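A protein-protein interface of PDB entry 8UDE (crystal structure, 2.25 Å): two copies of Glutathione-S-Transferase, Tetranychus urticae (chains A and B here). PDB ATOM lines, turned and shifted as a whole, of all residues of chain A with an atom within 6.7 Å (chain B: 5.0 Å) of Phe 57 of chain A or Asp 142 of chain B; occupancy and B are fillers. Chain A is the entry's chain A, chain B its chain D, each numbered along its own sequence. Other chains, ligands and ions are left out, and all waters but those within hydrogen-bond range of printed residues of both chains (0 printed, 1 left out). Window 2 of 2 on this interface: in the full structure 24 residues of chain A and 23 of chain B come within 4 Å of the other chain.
CD1 of Phe 146 of chain B touches CG of Asp 56 of chain A (3.6 Å).
Met 101 of chain B touches Phe 57 of chain A.
Phe 57 of chain A touches Asp 142 of chain B.
CB of Phe 146 of chain B touches CZ of Phe 57 of chain A, at 3.6 Å.
OG1 of Thr 73 of chain A touches CE of Met 101 of chain B (3.0 Å).
Met 101 of chain B touches Gln 74 of chain A (O to CG, 3.9 Å).
Of the 12 printed residues of chain A, 4 touch a printed residue of chain B.
Printed residues of chain B that touch a printed residue of chain A: Met 101, Gln 105, Asp 142 and Phe 146.
Hydrophobic or aromatic side chains of chain B within 4 Å of the printed part of chain A: Met 101 and Phe 146.
No position is printed for both chains.
Of the 7 pairs that touch across the chains among the printed residues, none has its exchanged pair printed and touching as well.
The backbone carbonyl oxygen (O) of Phe 57 of chain A lies within hydrogen-bond range of the side-chain hydroxyl (OG1) of Thr 73 of chain A (2.8 Å).
The side-chain hydroxyl (OG1) of Thr 73 of chain A sits at hydrogen-bond distance from the side-chain amide nitrogen (NE2) of Gln 74 of chain A (3.2 Å).
The side-chain amide nitrogen (NE2) of Gln 105 of chain B sits at hydrogen-bond distance from the side-chain amide oxygen (OE1) of Gln 74 of chain A (3.0 Å).
Of chain B, only Met 101, Asp 142 and Phe 146 come within 4 Å of Phe 57 of chain A.
Printed residues of chain B within 4 Å of Thr 73 of chain A: Met 101 (3.0 Å).
Printed residues of chain A within 4 Å of Met 101 of chain B: Phe 57, Thr 73 and Gln 74.
Of chain A, only Phe 57 comes within 4 Å of Asp 142 of chain B.
Of the printed residues of chain A, Phe 146 of chain B touches Asp 56 (3.6 Å) and Phe 57 (3.6 Å).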
ATOM      1  N   TRP A  46     -21.755 -37.053  -9.411  1.00  0.00           N
ATOM      2  CA  TRP A  46     -22.404 -36.109 -10.318  1.00  0.00           C
ATOM      3  C   TRP A  46     -21.509 -35.808 -11.532  1.00  0.00           C
ATOM      4  O   TRP A  46     -21.950 -35.821 -12.673  1.00  0.00           O
ATOM      5  CB  TRP A  46     -22.781 -34.813  -9.582  1.00  0.00           C
ATOM      6  CG  TRP A  46     -23.253 -33.685 -10.477  1.00  0.00           C
ATOM      7  CD1 TRP A  46     -22.829 -32.390 -10.424  1.00  0.00           C
ATOM      8  CD2 TRP A  46     -24.209 -33.748 -11.570  1.00  0.00           C
ATOM      9  NE1 TRP A  46     -23.464 -31.644 -11.378  1.00  0.00           N
ATOM     10  CE2 TRP A  46     -24.305 -32.448 -12.101  1.00  0.00           C
ATOM     11  CE3 TRP A  46     -24.982 -34.762 -12.147  1.00  0.00           C
ATOM     12  CZ2 TRP A  46     -25.141 -32.141 -13.171  1.00  0.00           C
ATOM     13  CZ3 TRP A  46     -25.807 -34.453 -13.208  1.00  0.00           C
ATOM     14  CH2 TRP A  46     -25.892 -33.156 -13.707  1.00  0.00           C
ATOM     15  N   GLY A  54     -26.580 -35.408 -21.921  1.00  0.00           N
ATOM     16  CA  GLY A  54     -27.117 -34.705 -23.073  1.00  0.00           C
ATOM     17  C   GLY A  54     -27.888 -33.443 -22.679  1.00  0.00           C
ATOM     18  O   GLY A  54     -28.758 -32.996 -23.434  1.00  0.00           O
ATOM     19  N   LEU A  55     -27.567 -32.901 -21.500  1.00  0.00           N
ATOM     20  CA  LEU A  55     -28.188 -31.700 -20.947  1.00  0.00           C
ATOM     21  C   LEU A  55     -27.585 -30.452 -21.580  1.00  0.00           C
ATOM     22  O   LEU A  55     -26.371 -30.336 -21.658  1.00  0.00           O
ATOM     23  CB  LEU A  55     -27.922 -31.662 -19.435  1.00  0.00           C
ATOM     24  CG  LEU A  55     -28.583 -32.798 -18.644  1.00  0.00           C
ATOM     25  CD1 LEU A  55     -28.173 -32.741 -17.184  1.00  0.00           C
ATOM     26  CD2 LEU A  55     -30.112 -32.753 -18.773  1.00  0.00           C
ATOM     27  N   ASP A  56     -28.436 -29.482 -21.894  1.00  0.00           N
ATOM     28  CA  ASP A  56     -28.014 -28.233 -22.496  1.00  0.00           C
ATOM     29  C   ASP A  56     -27.286 -27.385 -21.466  1.00  0.00           C
ATOM     30  O   ASP A  56     -26.234 -26.823 -21.794  1.00  0.00           O
ATOM     31  CB  ASP A  56     -29.222 -27.509 -23.080  1.00  0.00           C
ATOM     32  CG  ASP A  56     -29.679 -28.143 -24.374  1.00  0.00           C
ATOM     33  OD1 ASP A  56     -28.857 -28.154 -25.346  1.00  0.00           O
ATOM     34  OD2 ASP A  56     -30.846 -28.578 -24.417  1.00  0.00           O
ATOM     35  N   PHE A  57     -27.874 -27.304 -20.260  1.00  0.00           N
ATOM     36  CA  PHE A  57     -27.336 -26.511 -19.167  1.00  0.00           C
ATOM     37  C   PHE A  57     -27.112 -27.434 -17.978  1.00  0.00           C
ATOM     38  O   PHE A  57     -27.959 -27.544 -17.096  1.00  0.00           O
ATOM     39  CB  PHE A  57     -28.261 -25.354 -18.824  1.00  0.00           C
ATOM     40  CG  PHE A  57     -28.470 -24.404 -19.976  1.00  0.00           C
ATOM     41  CD1 PHE A  57     -27.513 -23.473 -20.312  1.00  0.00           C
ATOM     42  CD2 PHE A  57     -29.619 -24.455 -20.734  1.00  0.00           C
ATOM     43  CE1 PHE A  57     -27.712 -22.598 -21.365  1.00  0.00           C
ATOM     44  CE2 PHE A  57     -29.806 -23.600 -21.811  1.00  0.00           C
ATOM     45  CZ  PHE A  57     -28.855 -22.668 -22.123  1.00  0.00           C
ATOM     46  N   PRO A  58     -25.990 -28.184 -17.955  1.00  0.00           N
ATOM     47  CA  PRO A  58     -25.876 -29.343 -17.074  1.00  0.00           C
ATOM     48  C   PRO A  58     -25.902 -28.810 -15.652  1.00  0.00           C
ATOM     49  O   PRO A  58     -25.118 -27.954 -15.302  1.00  0.00           O
ATOM     50  CB  PRO A  58     -24.525 -29.970 -17.420  1.00  0.00           C
ATOM     51  CG  PRO A  58     -24.035 -29.267 -18.670  1.00  0.00           C
ATOM     52  CD  PRO A  58     -24.774 -27.949 -18.747  1.00  0.00           C
ATOM     53  N   ASN A  59     -26.868 -29.247 -14.868  1.00  0.00           N
ATOM     54  CA  ASN A  59     -27.009 -28.762 -13.512  1.00  0.00           C
ATOM     55  C   ASN A  59     -27.956 -29.696 -12.775  1.00  0.00           C
ATOM     56  O   ASN A  59     -28.644 -30.519 -13.403  1.00  0.00           O
ATOM     57  CB  ASN A  59     -27.527 -27.335 -13.516  1.00  0.00           C
ATOM     58  CG  ASN A  59     -27.096 -26.541 -12.300  1.00  0.00           C
ATOM     59  OD1 ASN A  59     -26.545 -27.078 -11.336  1.00  0.00           O
ATOM     60  ND2 ASN A  59     -27.428 -25.266 -12.291  1.00  0.00           N
ATOM     61  N   LEU A  60     -27.983 -29.561 -11.440  1.00  0.00           N
ATOM     62  CA  LEU A  60     -29.016 -30.227 -10.670  1.00  0.00           C
ATOM     63  C   LEU A  60     -29.977 -29.192 -10.089  1.00  0.00           C
ATOM     64  O   LEU A  60     -29.563 -28.158  -9.609  1.00  0.00           O
ATOM     65  CB  LEU A  60     -28.348 -31.083  -9.605  1.00  0.00           C
ATOM     66  CG  LEU A  60     -27.544 -32.277 -10.095  1.00  0.00           C
ATOM     67  CD1 LEU A  60     -26.763 -32.892  -8.936  1.00  0.00           C
ATOM     68  CD2 LEU A  60     -28.452 -33.285 -10.718  1.00  0.00           C
ATOM     69  N   PRO A  61     -31.307 -29.417 -10.091  1.00  0.00           N
ATOM     70  CA  PRO A  61     -31.901 -30.650 -10.605  1.00  0.00           C
ATOM     71  C   PRO A  61     -31.971 -30.796 -12.128  1.00  0.00           C
ATOM     72  O   PRO A  61     -31.946 -29.825 -12.872  1.00  0.00           O
ATOM     73  CB  PRO A  61     -33.339 -30.595 -10.044  1.00  0.00           C
ATOM     74  CG  PRO A  61     -33.626 -29.108  -9.949  1.00  0.00           C
ATOM     75  CD  PRO A  61     -32.307 -28.467  -9.572  1.00  0.00           C
ATOM     76  N   ILE A  72     -34.520 -31.649 -19.176  1.00  0.00           N
ATOM     77  CA  ILE A  72     -34.767 -30.331 -18.620  1.00  0.00           C
ATOM     78  C   ILE A  72     -33.849 -30.107 -17.429  1.00  0.00           C
ATOM     79  O   ILE A  72     -33.798 -30.956 -16.555  1.00  0.00           O
ATOM     80  CB  ILE A  72     -36.233 -30.120 -18.187  1.00  0.00           C
ATOM     81  CG1 ILE A  72     -37.248 -30.666 -19.192  1.00  0.00           C
ATOM     82  CG2 ILE A  72     -36.475 -28.637 -17.928  1.00  0.00           C
ATOM     83  CD1 ILE A  72     -38.702 -30.567 -18.727  1.00  0.00           C
ATOM     84  N   THR A  73     -33.287 -28.897 -17.351  1.00  0.00           N
ATOM     85  CA  THR A  73     -32.563 -28.454 -16.133  1.00  0.00           C
ATOM     86  C   THR A  73     -33.258 -27.131 -15.783  1.00  0.00           C
ATOM     87  O   THR A  73     -34.204 -26.795 -16.519  1.00  0.00           O
ATOM     88  CB  THR A  73     -31.046 -28.358 -16.338  1.00  0.00           C
ATOM     89  OG1 THR A  73     -30.762 -27.240 -17.178  1.00  0.00           O
ATOM     90  CG2 THR A  73     -30.451 -29.619 -16.927  1.00  0.00           C
ATOM     91  N   GLN A  74     -32.835 -26.415 -14.736  1.00  0.00           N
ATOM     92  CA  GLN A  74     -33.506 -25.156 -14.287  1.00  0.00           C
ATOM     93  C   GLN A  74     -34.813 -25.507 -13.562  1.00  0.00           C
ATOM     94  O   GLN A  74     -35.784 -25.875 -14.246  1.00  0.00           O
ATOM     95  CB  GLN A  74     -33.726 -24.169 -15.440  1.00  0.00           C
ATOM     96  CG  GLN A  74     -32.518 -23.987 -16.350  1.00  0.00           C
ATOM     97  CD  GLN A  74     -31.270 -23.583 -15.605  1.00  0.00           C
ATOM     98  OE1 GLN A  74     -31.207 -22.523 -14.988  1.00  0.00           O
ATOM     99  NE2 GLN A  74     -30.255 -24.429 -15.672  1.00  0.00           N
ATOM    100  N   MET B 101     -35.969 -22.568 -19.996  1.00  0.00           N
ATOM    101  CA  MET B 101     -34.615 -22.785 -19.494  1.00  0.00           C
ATOM    102  C   MET B 101     -33.808 -21.494 -19.686  1.00  0.00           C
ATOM    103  O   MET B 101     -33.158 -21.026 -18.772  1.00  0.00           O
ATOM    104  CB  MET B 101     -33.891 -23.968 -20.159  1.00  0.00           C
ATOM    105  CG  MET B 101     -34.377 -25.327 -19.699  1.00  0.00           C
ATOM    106  SD  MET B 101     -33.596 -26.759 -20.481  1.00  0.00           S
ATOM    107  CE  MET B 101     -31.921 -26.599 -19.904  1.00  0.00           C
ATOM    108  N   VAL B 102     -33.854 -20.895 -20.882  1.00  0.00           N
ATOM    109  CA  VAL B 102     -33.046 -19.722 -21.155  1.00  0.00           C
ATOM    110  C   VAL B 102     -33.527 -18.557 -20.281  1.00  0.00           C
ATOM    111  O   VAL B 102     -32.737 -17.717 -19.835  1.00  0.00           O
ATOM    112  CB  VAL B 102     -33.072 -19.382 -22.651  1.00  0.00           C
ATOM    113  CG1 VAL B 102     -32.343 -18.080 -22.966  1.00  0.00           C
ATOM    114  CG2 VAL B 102     -32.464 -20.500 -23.464  1.00  0.00           C
ATOM    115  N   GLN B 105     -31.887 -18.721 -16.930  1.00  0.00           N
ATOM    116  CA  GLN B 105     -30.512 -18.260 -17.084  1.00  0.00           C
ATOM    117  C   GLN B 105     -30.476 -16.726 -17.129  1.00  0.00           C
ATOM    118  O   GLN B 105     -29.713 -16.088 -16.398  1.00  0.00           O
ATOM    119  CB  GLN B 105     -29.863 -18.847 -18.333  1.00  0.00           C
ATOM    120  CG  GLN B 105     -29.426 -20.302 -18.203  1.00  0.00           C
ATOM    121  CD  GLN B 105     -28.356 -20.472 -17.159  1.00  0.00           C
ATOM    122  OE1 GLN B 105     -27.290 -19.853 -17.169  1.00  0.00           O
ATOM    123  NE2 GLN B 105     -28.685 -21.299 -16.189  1.00  0.00           N
ATOM    124  N   ARG B 138     -18.079 -19.119 -18.488  1.00  0.00           N
ATOM    125  CA  ARG B 138     -18.689 -20.429 -18.670  1.00  0.00           C
ATOM    126  C   ARG B 138     -20.165 -20.309 -19.035  1.00  0.00           C
ATOM    127  O   ARG B 138     -20.639 -21.042 -19.895  1.00  0.00           O
ATOM    128  CB  ARG B 138     -18.573 -21.289 -17.407  1.00  0.00           C
ATOM    129  CG  ARG B 138     -19.014 -22.720 -17.646  1.00  0.00           C
ATOM    130  CD  ARG B 138     -18.456 -23.665 -16.609  1.00  0.00           C
ATOM    131  NE  ARG B 138     -18.606 -25.051 -17.030  1.00  0.00           N
ATOM    132  CZ  ARG B 138     -18.486 -26.114 -16.224  1.00  0.00           C
ATOM    133  NH1 ARG B 138     -18.587 -27.343 -16.703  1.00  0.00           N
ATOM    134  NH2 ARG B 138     -18.258 -25.951 -14.933  1.00  0.00           N
ATOM    135  N   LYS B 139     -20.901 -19.442 -18.332  1.00  0.00           N
ATOM    136  CA  LYS B 139     -22.339 -19.280 -18.578  1.00  0.00           C
ATOM    137  C   LYS B 139     -22.626 -18.730 -19.978  1.00  0.00           C
ATOM    138  O   LYS B 139     -23.627 -19.106 -20.598  1.00  0.00           O
ATOM    139  CB  LYS B 139     -23.007 -18.377 -17.537  1.00  0.00           C
ATOM    140  CG  LYS B 139     -23.079 -18.956 -16.119  1.00  0.00           C
ATOM    141  CD  LYS B 139     -23.633 -17.957 -15.118  1.00  0.00           C
ATOM    142  CE  LYS B 139     -24.001 -18.563 -13.779  1.00  0.00           C
ATOM    143  NZ  LYS B 139     -22.780 -18.872 -13.002  1.00  0.00           N
ATOM    144  N   LEU B 140     -21.738 -17.879 -20.482  1.00  0.00           N
ATOM    145  CA  LEU B 140     -21.876 -17.317 -21.813  1.00  0.00           C
ATOM    146  C   LEU B 140     -21.557 -18.372 -22.863  1.00  0.00           C
ATOM    147  O   LEU B 140     -22.200 -18.416 -23.906  1.00  0.00           O
ATOM    148  CB  LEU B 140     -20.951 -16.102 -21.936  1.00  0.00           C
ATOM    149  CG  LEU B 140     -21.369 -14.924 -21.071  1.00  0.00           C
ATOM    150  CD1 LEU B 140     -20.361 -13.798 -21.161  1.00  0.00           C
ATOM    151  CD2 LEU B 140     -22.751 -14.438 -21.497  1.00  0.00           C
ATOM    152  N   ILE B 141     -20.564 -19.225 -22.569  1.00  0.00           N
ATOM    153  CA  ILE B 141     -20.249 -20.340 -23.457  1.00  0.00           C
ATOM    154  C   ILE B 141     -21.470 -21.269 -23.562  1.00  0.00           C
ATOM    155  O   ILE B 141     -21.874 -21.663 -24.648  1.00  0.00           O
ATOM    156  CB  ILE B 141     -18.986 -21.080 -22.973  1.00  0.00           C
ATOM    157  CG1 ILE B 141     -17.737 -20.237 -23.218  1.00  0.00           C
ATOM    158  CG2 ILE B 141     -18.881 -22.457 -23.611  1.00  0.00           C
ATOM    159  CD1 ILE B 141     -16.469 -20.791 -22.566  1.00  0.00           C
ATOM    160  N   ASP B 142     -22.104 -21.576 -22.429  1.00  0.00           N
ATOM    161  CA  ASP B 142     -23.233 -22.480 -22.425  1.00  0.00           C
ATOM    162  C   ASP B 142     -24.381 -21.882 -23.250  1.00  0.00           C
ATOM    163  O   ASP B 142     -25.026 -22.598 -24.004  1.00  0.00           O
ATOM    164  CB  ASP B 142     -23.656 -22.820 -21.003  1.00  0.00           C
ATOM    165  CG  ASP B 142     -22.711 -23.736 -20.235  1.00  0.00           C
ATOM    166  OD1 ASP B 142     -21.940 -24.470 -20.868  1.00  0.00           O
ATOM    167  OD2 ASP B 142     -22.739 -23.675 -18.980  1.00  0.00           O
ATOM    168  N   LEU B 143     -24.634 -20.575 -23.094  1.00  0.00           N
ATOM    169  CA  LEU B 143     -25.642 -19.877 -23.885  1.00  0.00           C
ATOM    170  C   LEU B 143     -25.300 -19.901 -25.375  1.00  0.00           C
ATOM    171  O   LEU B 143     -26.185 -20.164 -26.188  1.00  0.00           O
ATOM    172  CB  LEU B 143     -25.747 -18.444 -23.352  1.00  0.00           C
ATOM    173  CG  LEU B 143     -26.591 -18.278 -22.092  1.00  0.00           C
ATOM    174  CD1 LEU B 143     -26.321 -16.953 -21.391  1.00  0.00           C
ATOM    175  CD2 LEU B 143     -28.070 -18.407 -22.440  1.00  0.00           C
ATOM    176  N   ALA B 144     -24.018 -19.640 -25.731  1.00  0.00           N
ATOM    177  CA  ALA B 144     -23.621 -19.679 -27.124  1.00  0.00           C
ATOM    178  C   ALA B 144     -23.850 -21.057 -27.718  1.00  0.00           C
ATOM    179  O   ALA B 144     -24.353 -21.161 -28.845  1.00  0.00           O
ATOM    180  CB  ALA B 144     -22.190 -19.264 -27.282  1.00  0.00           C
ATOM    181  N   LYS B 145     -23.437 -22.093 -26.969  1.00  0.00           N
ATOM    182  CA  LYS B 145     -23.620 -23.472 -27.424  1.00  0.00           C
ATOM    183  C   LYS B 145     -25.104 -23.793 -27.614  1.00  0.00           C
ATOM    184  O   LYS B 145     -25.457 -24.514 -28.531  1.00  0.00           O
ATOM    185  CB  LYS B 145     -23.119 -24.516 -26.422  1.00  0.00           C
ATOM    186  CG  LYS B 145     -21.619 -24.596 -26.220  1.00  0.00           C
ATOM    187  CD  LYS B 145     -21.233 -25.583 -25.129  1.00  0.00           C
ATOM    188  CE  LYS B 145     -21.591 -27.026 -25.425  1.00  0.00           C
ATOM    189  NZ  LYS B 145     -21.156 -27.866 -24.284  1.00  0.00           N
ATOM    190  N   PHE B 146     -25.970 -23.283 -26.732  1.00  0.00           N
ATOM    191  CA  PHE B 146     -27.391 -23.557 -26.850  1.00  0.00           C
ATOM    192  C   PHE B 146     -27.929 -22.873 -28.108  1.00  0.00           C
ATOM    193  O   PHE B 146     -28.737 -23.454 -28.802  1.00  0.00           O
ATOM    194  CB  PHE B 146     -28.181 -23.100 -25.612  1.00  0.00           C
ATOM    195  CG  PHE B 146     -29.645 -23.450 -25.662  1.00  0.00           C
ATOM    196  CD1 PHE B 146     -30.080 -24.720 -25.303  1.00  0.00           C
ATOM    197  CD2 PHE B 146     -30.583 -22.555 -26.157  1.00  0.00           C
ATOM    198  CE1 PHE B 146     -31.423 -25.070 -25.379  1.00  0.00           C
ATOM    199  CE2 PHE B 146     -31.923 -22.910 -26.238  1.00  0.00           C
ATOM    200  CZ  PHE B 146     -32.340 -24.155 -25.831  1.00  0.00           C
